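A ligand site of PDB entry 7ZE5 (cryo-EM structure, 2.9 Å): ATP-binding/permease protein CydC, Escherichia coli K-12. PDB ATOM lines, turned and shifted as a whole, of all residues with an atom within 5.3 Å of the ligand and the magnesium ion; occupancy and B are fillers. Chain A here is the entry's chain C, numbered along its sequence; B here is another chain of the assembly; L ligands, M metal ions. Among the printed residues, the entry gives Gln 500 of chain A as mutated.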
ATOM      1  N   TYR A 348      -3.205  11.309   8.607  1.00  0.00           N
ATOM      2  CA  TYR A 348      -3.188  10.082   7.839  1.00  0.00           C
ATOM      3  C   TYR A 348      -4.416  10.023   6.932  1.00  0.00           C
ATOM      4  O   TYR A 348      -5.444  10.648   7.224  1.00  0.00           O
ATOM      5  CB  TYR A 348      -3.150   8.869   8.770  1.00  0.00           C
ATOM      6  CG  TYR A 348      -1.749   8.443   9.140  1.00  0.00           C
ATOM      7  CD1 TYR A 348      -0.941   7.807   8.230  1.00  0.00           C
ATOM      8  CD2 TYR A 348      -1.252   8.678  10.410  1.00  0.00           C
ATOM      9  CE1 TYR A 348       0.336   7.413   8.565  1.00  0.00           C
ATOM     10  CE2 TYR A 348       0.019   8.288  10.757  1.00  0.00           C
ATOM     11  CZ  TYR A 348       0.807   7.657   9.834  1.00  0.00           C
ATOM     12  OH  TYR A 348       2.078   7.267  10.181  1.00  0.00           O
ATOM     13  N   PRO A 349      -4.330   9.305   5.817  1.00  0.00           N
ATOM     14  CA  PRO A 349      -5.461   9.262   4.884  1.00  0.00           C
ATOM     15  C   PRO A 349      -6.724   8.743   5.545  1.00  0.00           C
ATOM     16  O   PRO A 349      -6.693   7.820   6.353  1.00  0.00           O
ATOM     17  CB  PRO A 349      -4.975   8.323   3.780  1.00  0.00           C
ATOM     18  CG  PRO A 349      -3.497   8.430   3.842  1.00  0.00           C
ATOM     19  CD  PRO A 349      -3.162   8.575   5.292  1.00  0.00           C
ATOM     20  N   GLN A 351      -8.627  10.148   7.751  1.00  0.00           N
ATOM     21  CA  GLN A 351      -8.641  10.408   9.192  1.00  0.00           C
ATOM     22  C   GLN A 351      -8.999  11.870   9.436  1.00  0.00           C
ATOM     23  O   GLN A 351      -8.748  12.738   8.608  1.00  0.00           O
ATOM     24  CB  GLN A 351      -7.285  10.085   9.840  1.00  0.00           C
ATOM     25  CG  GLN A 351      -6.792   8.677   9.587  1.00  0.00           C
ATOM     26  CD  GLN A 351      -7.612   7.638  10.304  1.00  0.00           C
ATOM     27  OE1 GLN A 351      -8.186   7.906  11.359  1.00  0.00           O
ATOM     28  NE2 GLN A 351      -7.671   6.446   9.733  1.00  0.00           N
ATOM     29  N   ALA A 355      -1.982  13.101  13.188  1.00  0.00           N
ATOM     30  CA  ALA A 355      -0.920  12.302  13.775  1.00  0.00           C
ATOM     31  C   ALA A 355       0.255  13.172  14.203  1.00  0.00           C
ATOM     32  O   ALA A 355       0.900  12.881  15.210  1.00  0.00           O
ATOM     33  CB  ALA A 355      -0.453  11.243  12.787  1.00  0.00           C
ATOM     34  N   ARG A 374       5.048   8.164  24.580  1.00  0.00           N
ATOM     35  CA  ARG A 374       4.194   7.010  24.737  1.00  0.00           C
ATOM     36  C   ARG A 374       3.939   6.352  23.376  1.00  0.00           C
ATOM     37  O   ARG A 374       4.284   6.892  22.321  1.00  0.00           O
ATOM     38  CB  ARG A 374       2.863   7.385  25.379  1.00  0.00           C
ATOM     39  CG  ARG A 374       2.954   7.821  26.825  1.00  0.00           C
ATOM     40  CD  ARG A 374       1.569   8.086  27.394  1.00  0.00           C
ATOM     41  NE  ARG A 374       0.965   9.273  26.802  1.00  0.00           N
ATOM     42  CZ  ARG A 374      -0.105   9.243  26.008  1.00  0.00           C
ATOM     43  NH1 ARG A 374      -0.683   8.082  25.727  1.00  0.00           N
ATOM     44  NH2 ARG A 374      -0.600  10.365  25.511  1.00  0.00           N
ATOM     45  N   THR A 375       3.336   5.173  23.428  1.00  0.00           N
ATOM     46  CA  THR A 375       2.980   4.478  22.198  1.00  0.00           C
ATOM     47  C   THR A 375       1.830   5.197  21.511  1.00  0.00           C
ATOM     48  O   THR A 375       0.846   5.568  22.153  1.00  0.00           O
ATOM     49  CB  THR A 375       2.602   3.037  22.510  1.00  0.00           C
ATOM     50  OG1 THR A 375       1.462   3.015  23.366  1.00  0.00           O
ATOM     51  CG2 THR A 375       3.746   2.340  23.194  1.00  0.00           C
ATOM     52  N   GLY A 376       1.948   5.380  20.197  1.00  0.00           N
ATOM     53  CA  GLY A 376       0.930   6.085  19.454  1.00  0.00           C
ATOM     54  C   GLY A 376       1.057   7.590  19.476  1.00  0.00           C
ATOM     55  O   GLY A 376       0.074   8.284  19.189  1.00  0.00           O
ATOM     56  N   CYS A 377       2.225   8.119  19.811  1.00  0.00           N
ATOM     57  CA  CYS A 377       2.446   9.555  19.888  1.00  0.00           C
ATOM     58  C   CYS A 377       3.038  10.130  18.609  1.00  0.00           C
ATOM     59  O   CYS A 377       3.330  11.329  18.564  1.00  0.00           O
ATOM     60  CB  CYS A 377       3.339   9.892  21.087  1.00  0.00           C
ATOM     61  SG  CYS A 377       5.082   9.612  20.793  1.00  0.00           S
ATOM     62  N   GLY A 378       3.227   9.311  17.581  1.00  0.00           N
ATOM     63  CA  GLY A 378       3.735   9.807  16.321  1.00  0.00           C
ATOM     64  C   GLY A 378       5.233   9.751  16.159  1.00  0.00           C
ATOM     65  O   GLY A 378       5.794  10.564  15.409  1.00  0.00           O
ATOM     66  N   LYS A 379       5.909   8.817  16.824  1.00  0.00           N
ATOM     67  CA  LYS A 379       7.358   8.715  16.707  1.00  0.00           C
ATOM     68  C   LYS A 379       7.769   8.155  15.349  1.00  0.00           C
ATOM     69  O   LYS A 379       8.667   8.690  14.692  1.00  0.00           O
ATOM     70  CB  LYS A 379       7.922   7.845  17.834  1.00  0.00           C
ATOM     71  CG  LYS A 379       7.977   8.535  19.176  1.00  0.00           C
ATOM     72  CD  LYS A 379       8.727   7.688  20.198  1.00  0.00           C
ATOM     73  CE  LYS A 379       8.127   6.303  20.313  1.00  0.00           C
ATOM     74  NZ  LYS A 379       6.664   6.357  20.528  1.00  0.00           N
ATOM     75  N   SER A 380       7.121   7.077  14.922  1.00  0.00           N
ATOM     76  CA  SER A 380       7.445   6.493  13.623  1.00  0.00           C
ATOM     77  C   SER A 380       6.846   7.309  12.493  1.00  0.00           C
ATOM     78  O   SER A 380       7.383   7.316  11.369  1.00  0.00           O
ATOM     79  CB  SER A 380       6.964   5.046  13.547  1.00  0.00           C
ATOM     80  OG  SER A 380       7.545   4.252  14.568  1.00  0.00           O
ATOM     81  N   THR A 381       5.734   7.988  12.748  1.00  0.00           N
ATOM     82  CA  THR A 381       5.161   8.885  11.751  1.00  0.00           C
ATOM     83  C   THR A 381       6.117  10.017  11.431  1.00  0.00           C
ATOM     84  O   THR A 381       6.275  10.414  10.266  1.00  0.00           O
ATOM     85  CB  THR A 381       3.815   9.426  12.235  1.00  0.00           C
ATOM     86  OG1 THR A 381       2.836   8.383  12.191  1.00  0.00           O
ATOM     87  CG2 THR A 381       3.353  10.564  11.360  1.00  0.00           C
ATOM     88  N   LEU A 382       6.784  10.556  12.454  1.00  0.00           N
ATOM     89  CA  LEU A 382       7.789  11.585  12.241  1.00  0.00           C
ATOM     90  C   LEU A 382       8.948  11.061  11.408  1.00  0.00           C
ATOM     91  O   LEU A 382       9.419  11.725  10.486  1.00  0.00           O
ATOM     92  CB  LEU A 382       8.284  12.118  13.580  1.00  0.00           C
ATOM     93  CG  LEU A 382       9.421  13.126  13.505  1.00  0.00           C
ATOM     94  CD1 LEU A 382       8.993  14.319  12.690  1.00  0.00           C
ATOM     95  CD2 LEU A 382       9.852  13.557  14.889  1.00  0.00           C
ATOM     96  N   GLN A 421      10.961   0.045  12.583  1.00  0.00           N
ATOM     97  CA  GLN A 421      10.504  -0.658  13.766  1.00  0.00           C
ATOM     98  C   GLN A 421      10.207  -2.116  13.461  1.00  0.00           C
ATOM     99  O   GLN A 421      10.511  -3.000  14.273  1.00  0.00           O
ATOM    100  CB  GLN A 421       9.271   0.027  14.345  1.00  0.00           C
ATOM    101  CG  GLN A 421       8.953  -0.393  15.762  1.00  0.00           C
ATOM    102  CD  GLN A 421       8.111   0.614  16.493  1.00  0.00           C
ATOM    103  OE1 GLN A 421       7.755   1.660  15.953  1.00  0.00           O
ATOM    104  NE2 GLN A 421       7.764   0.301  17.728  1.00  0.00           N
ATOM    105  N   ASP A 499      14.674   3.522  14.489  1.00  0.00           N
ATOM    106  CA  ASP A 499      13.339   3.384  15.072  1.00  0.00           C
ATOM    107  C   ASP A 499      13.358   2.180  16.015  1.00  0.00           C
ATOM    108  O   ASP A 499      13.119   1.044  15.596  1.00  0.00           O
ATOM    109  CB  ASP A 499      12.287   3.217  13.986  1.00  0.00           C
ATOM    110  CG  ASP A 499      10.894   3.594  14.451  1.00  0.00           C
ATOM    111  OD1 ASP A 499      10.689   3.691  15.677  1.00  0.00           O
ATOM    112  OD2 ASP A 499      10.014   3.778  13.597  1.00  0.00           O
ATOM    113  N   GLN A 500      13.631   2.445  17.295  1.00  0.00           N
ATOM    114  CA  GLN A 500      13.788   1.411  18.305  1.00  0.00           C
ATOM    115  C   GLN A 500      14.762   0.315  17.848  1.00  0.00           C
ATOM    116  O   GLN A 500      14.356  -0.842  17.668  1.00  0.00           O
ATOM    117  CB  GLN A 500      12.438   0.822  18.697  1.00  0.00           C
ATOM    118  CG  GLN A 500      11.581   1.812  19.450  1.00  0.00           C
ATOM    119  CD  GLN A 500      10.120   1.440  19.492  1.00  0.00           C
ATOM    120  OE1 GLN A 500       9.266   2.224  19.098  1.00  0.00           O
ATOM    121  NE2 GLN A 500       9.831   0.245  19.971  1.00  0.00           N
ATOM    122  N   HIS A 531      11.880   3.415  23.197  1.00  0.00           N
ATOM    123  CA  HIS A 531      11.211   3.436  24.491  1.00  0.00           C
ATOM    124  C   HIS A 531      12.170   3.084  25.621  1.00  0.00           C
ATOM    125  O   HIS A 531      11.749   3.066  26.779  1.00  0.00           O
ATOM    126  CB  HIS A 531      10.023   2.465  24.493  1.00  0.00           C
ATOM    127  CG  HIS A 531       8.924   2.864  23.564  1.00  0.00           C
ATOM    128  ND1 HIS A 531       8.718   2.243  22.351  1.00  0.00           N
ATOM    129  CD2 HIS A 531       7.982   3.836  23.658  1.00  0.00           C
ATOM    130  CE1 HIS A 531       7.678   2.803  21.756  1.00  0.00           C
ATOM    131  NE2 HIS A 531       7.214   3.773  22.522  1.00  0.00           N
ATOM    132  N   LEU B 470      -9.012   7.702  19.577  1.00  0.00           N
ATOM    133  CA  LEU B 470      -8.305   8.146  18.382  1.00  0.00           C
ATOM    134  C   LEU B 470      -8.780   7.415  17.138  1.00  0.00           C
ATOM    135  O   LEU B 470      -8.726   7.963  16.030  1.00  0.00           O
ATOM    136  CB  LEU B 470      -6.801   7.956  18.556  1.00  0.00           C
ATOM    137  CG  LEU B 470      -6.025   8.965  19.407  1.00  0.00           C
ATOM    138  CD1 LEU B 470      -6.327   8.831  20.890  1.00  0.00           C
ATOM    139  CD2 LEU B 470      -4.528   8.822  19.163  1.00  0.00           C
ATOM    140  N   LEU B 471      -9.250   6.175  17.282  1.00  0.00           N
ATOM    141  CA  LEU B 471      -9.703   5.413  16.143  1.00  0.00           C
ATOM    142  C   LEU B 471     -11.039   5.957  15.631  1.00  0.00           C
ATOM    143  O   LEU B 471     -11.898   6.331  16.432  1.00  0.00           O
ATOM    144  CB  LEU B 471      -9.837   3.939  16.507  1.00  0.00           C
ATOM    145  CG  LEU B 471      -8.570   3.255  17.030  1.00  0.00           C
ATOM    146  CD1 LEU B 471      -8.793   1.769  17.157  1.00  0.00           C
ATOM    147  CD2 LEU B 471      -7.390   3.536  16.127  1.00  0.00           C
ATOM    148  N   ALA B 484      -1.630  -2.322   9.535  1.00  0.00           N
ATOM    149  CA  ALA B 484      -1.069  -1.048   9.105  1.00  0.00           C
ATOM    150  C   ALA B 484      -1.699   0.120   9.846  1.00  0.00           C
ATOM    151  O   ALA B 484      -1.026   1.115  10.129  1.00  0.00           O
ATOM    152  CB  ALA B 484      -1.240  -0.883   7.596  1.00  0.00           C
ATOM    153  N   ARG B 485      -2.990   0.018  10.169  1.00  0.00           N
ATOM    154  CA  ARG B 485      -3.695   1.136  10.783  1.00  0.00           C
ATOM    155  C   ARG B 485      -3.164   1.431  12.187  1.00  0.00           C
ATOM    156  O   ARG B 485      -3.232   2.581  12.634  1.00  0.00           O
ATOM    157  CB  ARG B 485      -5.197   0.836  10.831  1.00  0.00           C
ATOM    158  CG  ARG B 485      -6.021   1.801  11.660  1.00  0.00           C
ATOM    159  CD  ARG B 485      -5.994   3.191  11.062  1.00  0.00           C
ATOM    160  NE  ARG B 485      -6.698   4.172  11.893  1.00  0.00           N
ATOM    161  CZ  ARG B 485      -6.149   4.818  12.910  1.00  0.00           C
ATOM    162  NH1 ARG B 485      -4.886   4.603  13.234  1.00  0.00           N
ATOM    163  NH2 ARG B 485      -6.867   5.693  13.599  1.00  0.00           N
ATOM    164  N   LEU B 486      -2.621   0.430  12.866  1.00  0.00           N
ATOM    165  CA  LEU B 486      -2.103   0.608  14.214  1.00  0.00           C
ATOM    166  C   LEU B 486      -0.591   0.757  14.191  1.00  0.00           C
ATOM    167  O   LEU B 486       0.090   0.365  13.256  1.00  0.00           O
ATOM    168  CB  LEU B 486      -2.487  -0.584  15.091  1.00  0.00           C
ATOM    169  CG  LEU B 486      -3.950  -1.026  15.094  1.00  0.00           C
ATOM    170  CD1 LEU B 486      -4.090  -2.343  15.834  1.00  0.00           C
ATOM    171  CD2 LEU B 486      -4.825   0.028  15.727  1.00  0.00           C
ATOM    172  N   SER B 487      -0.073   1.351  15.266  1.00  0.00           N
ATOM    173  CA  SER B 487       1.365   1.346  15.490  1.00  0.00           C
ATOM    174  C   SER B 487       1.773   0.028  16.138  1.00  0.00           C
ATOM    175  O   SER B 487       0.940  -0.768  16.577  1.00  0.00           O
ATOM    176  CB  SER B 487       1.767   2.531  16.359  1.00  0.00           C
ATOM    177  OG  SER B 487       1.297   2.380  17.688  1.00  0.00           O
ATOM    178  N   VAL B 488       3.083  -0.205  16.185  1.00  0.00           N
ATOM    179  CA  VAL B 488       3.582  -1.473  16.719  1.00  0.00           C
ATOM    180  C   VAL B 488       3.204  -1.630  18.183  1.00  0.00           C
ATOM    181  O   VAL B 488       2.812  -2.720  18.625  1.00  0.00           O
ATOM    182  CB  VAL B 488       5.101  -1.579  16.500  1.00  0.00           C
ATOM    183  CG1 VAL B 488       5.584  -2.961  16.875  1.00  0.00           C
ATOM    184  CG2 VAL B 488       5.441  -1.282  15.056  1.00  0.00           C
ATOM    185  N   GLY B 489       3.310  -0.556  18.956  1.00  0.00           N
ATOM    186  CA  GLY B 489       2.906  -0.628  20.356  1.00  0.00           C
ATOM    187  C   GLY B 489       1.424  -0.825  20.535  1.00  0.00           C
ATOM    188  O   GLY B 489       0.982  -1.512  21.463  1.00  0.00           O
ATOM    189  N   GLN B 490       0.616  -0.217  19.660  1.00  0.00           N
ATOM    190  CA  GLN B 490      -0.829  -0.405  19.748  1.00  0.00           C
ATOM    191  C   GLN B 490      -1.244  -1.787  19.281  1.00  0.00           C
ATOM    192  O   GLN B 490      -2.176  -2.381  19.829  1.00  0.00           O
ATOM    193  CB  GLN B 490      -1.549   0.677  18.932  1.00  0.00           C
ATOM    194  CG  GLN B 490      -1.292   2.084  19.422  1.00  0.00           C
ATOM    195  CD  GLN B 490      -2.105   3.109  18.680  1.00  0.00           C
ATOM    196  OE1 GLN B 490      -2.286   3.012  17.467  1.00  0.00           O
ATOM    197  NE2 GLN B 490      -2.604   4.101  19.403  1.00  0.00           N
ATOM    198  N   SER B 515       7.727  -2.894  22.332  1.00  0.00           N
ATOM    199  CA  SER B 515       7.277  -1.667  21.671  1.00  0.00           C
ATOM    200  C   SER B 515       6.390  -0.820  22.583  1.00  0.00           C
ATOM    201  O   SER B 515       5.577  -0.034  22.095  1.00  0.00           O
ATOM    202  CB  SER B 515       6.563  -1.978  20.355  1.00  0.00           C
ATOM    203  OG  SER B 515       7.452  -2.578  19.438  1.00  0.00           O
HETATM  204  P1  LIG L   1       4.933   3.107  18.800  1.00  0.00           P
HETATM  205  O1  LIG L   1       4.088   2.322  19.754  1.00  0.00           O
HETATM  206  O2  LIG L   1       5.943   4.005  19.472  1.00  0.00           O
HETATM  207  O3  LIG L   1       5.480   2.325  17.633  1.00  0.00           O
HETATM  208  P2  LIG L   1       4.464   5.343  17.229  1.00  0.00           P
HETATM  209  O4  LIG L   1       5.294   4.749  16.127  1.00  0.00           O
HETATM  210  O5  LIG L   1       5.065   6.358  18.158  1.00  0.00           O
HETATM  211  O6  LIG L   1       3.897   4.129  18.120  1.00  0.00           O
HETATM  212  P3  LIG L   1       2.947   6.107  15.003  1.00  0.00           P
HETATM  213  O7  LIG L   1       3.951   7.110  14.498  1.00  0.00           O
HETATM  214  O8  LIG L   1       2.931   4.728  14.412  1.00  0.00           O
HETATM  215  O9  LIG L   1       3.128   5.975  16.591  1.00  0.00           O
HETATM  216  O10 LIG L   1       1.496   6.758  14.872  1.00  0.00           O
HETATM  217  C1  LIG L   1       0.765   7.139  16.033  1.00  0.00           C
HETATM  218  C2  LIG L   1      -0.708   7.260  15.689  1.00  0.00           C
HETATM  219  O11 LIG L   1      -0.863   7.235  14.277  1.00  0.00           O
HETATM  220  C3  LIG L   1      -1.484   6.087  16.261  1.00  0.00           C
HETATM  221  O12 LIG L   1      -2.555   6.581  17.077  1.00  0.00           O
HETATM  222  C4  LIG L   1      -2.066   5.359  15.075  1.00  0.00           C
HETATM  223  O13 LIG L   1      -3.454   5.111  15.295  1.00  0.00           O
HETATM  224  C5  LIG L   1      -1.876   6.296  13.908  1.00  0.00           C
HETATM  225  N1  LIG L   1      -1.443   5.566  12.696  1.00  0.00           N
HETATM  226  C6  LIG L   1      -0.283   4.904  12.554  1.00  0.00           C
HETATM  227  N2  LIG L   1      -0.190   4.334  11.324  1.00  0.00           N
HETATM  228  C7  LIG L   1      -1.316   4.642  10.664  1.00  0.00           C
HETATM  229  C8  LIG L   1      -1.867   4.359   9.321  1.00  0.00           C
HETATM  230  N3  LIG L   1      -1.166   3.622   8.424  1.00  0.00           N
HETATM  231  N4  LIG L   1      -3.073   4.865   9.017  1.00  0.00           N
HETATM  232  C9  LIG L   1      -3.780   5.604   9.902  1.00  0.00           C
HETATM  233  N5  LIG L   1      -3.337   5.894  11.142  1.00  0.00           N
HETATM  234  C10 LIG L   1      -2.136   5.444  11.568  1.00  0.00           C
HETATM  235 MG    MG M   1       6.368   3.053  15.787  1.00  0.00          MG
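The backbone NH (N) of Ser 380 lies within hydrogen-bond range of an oxygen (O7) of the ligand, at 3.2 Å.
NH1 of Arg 485 of chain B is in hydrogen-bond range of O13 of the ligand, 2.6 Å away.
The backbone NH (N) of Thr 381 sits at hydrogen-bond distance from an oxygen (O7) of the ligand, 2.6 Å away.
The side-chain hydroxyl of Thr 381 is in hydrogen-bond range of an oxygen (O7) of the ligand, at 2.9 Å.
The backbone NH (N) of Lys 379 lies within hydrogen-bond range of an oxygen (O5) of the ligand, at 2.9 Å.
An oxygen (O2) of the ligand is in salt-bridge range of the side-chain amino group (NZ) of Lys 379 (2.7 Å).
The backbone carbonyl oxygen (O) of Ala 484 of chain B sits at hydrogen-bond distance from a nitrogen (N3) of the ligand (3.0 Å).
N of Gly 489 of chain B is in hydrogen-bond range of O1 of the ligand (3.1 Å).
NE2 of His 531 lies close to O2 of the ligand (3.3 Å).
O6 of the ligand is in hydrogen-bond range of N of Gly 376.
OG of Ser 487 of chain B lies within hydrogen-bond range of O6 of the ligand.
The side-chain amide oxygen of Gln 490 of chain B sits at hydrogen-bond distance from an oxygen (O13) of the ligand, 3.2 Å away.
N of Gly 378 sits at hydrogen-bond distance from O9 of the ligand (3.5 Å).
OE1 of Gln 500 sits at hydrogen-bond distance from NE2 of Gln 421 (2.8 Å).
The guanidinium group of Arg 485 of chain B lies close to the side-chain amide nitrogen of Gln 351 (3.3 Å).
OG1 of Thr 381 is in hydrogen-bond range of OH of Tyr 348 (2.4 Å).
A ring nitrogen (NE2) of His 531 is in hydrogen-bond range of the side-chain amino group (NZ) of Lys 379, at 3.3 Å.
NZ of Lys 379 sits close to SG of Cys 377, 3.6 Å away.
O of Arg 374 lies within hydrogen-bond range of NZ of Lys 379 (3.0 Å).
The side-chain amide oxygen of Gln 500 lies close to a ring nitrogen (ND1) of His 531 (3.3 Å).
The side-chain sulfur (SG) of Cys 377 sits at hydrogen-bond distance from the backbone carbonyl oxygen (O) of Arg 374.
Residues that only touch the ligand: Tyr 348 (3.5 Å), Gln 351 (3.98 Å), Thr 375 (3.2 Å), Cys 377 (3.7 Å), Gln 500 (3.8 Å), Leu 470 of chain B (3.6 Å), Val 488 of chain B (3.8 Å) and Ser 515 of chain B (3.6 Å).
Hydrophobic or aromatic side chains within 4 Å of the ligand: Tyr 348, His 531 and Leu 470 of chain B.
Of the 27 residues printed, 20 come within 4 Å of the ligand.
Along chain A the residues within 4 Å of the ligand span positions 348 to 531.
The nearest printed residue that does not touch the ligand is Arg 374 (4.3 Å).
The nearest printed residue that does not touch the magnesium ion is Asp 499 (4.3 Å).
OE1 of Gln 421 binds the magnesium ion, at 2.0 Å.
O4 of the ligand is bound to the magnesium ion (2.0 Å).
OG of Ser 380 binds the magnesium ion (2.1 Å).
An oxygen (O3) of the ligand binds the magnesium ion, 2.2 Å away.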
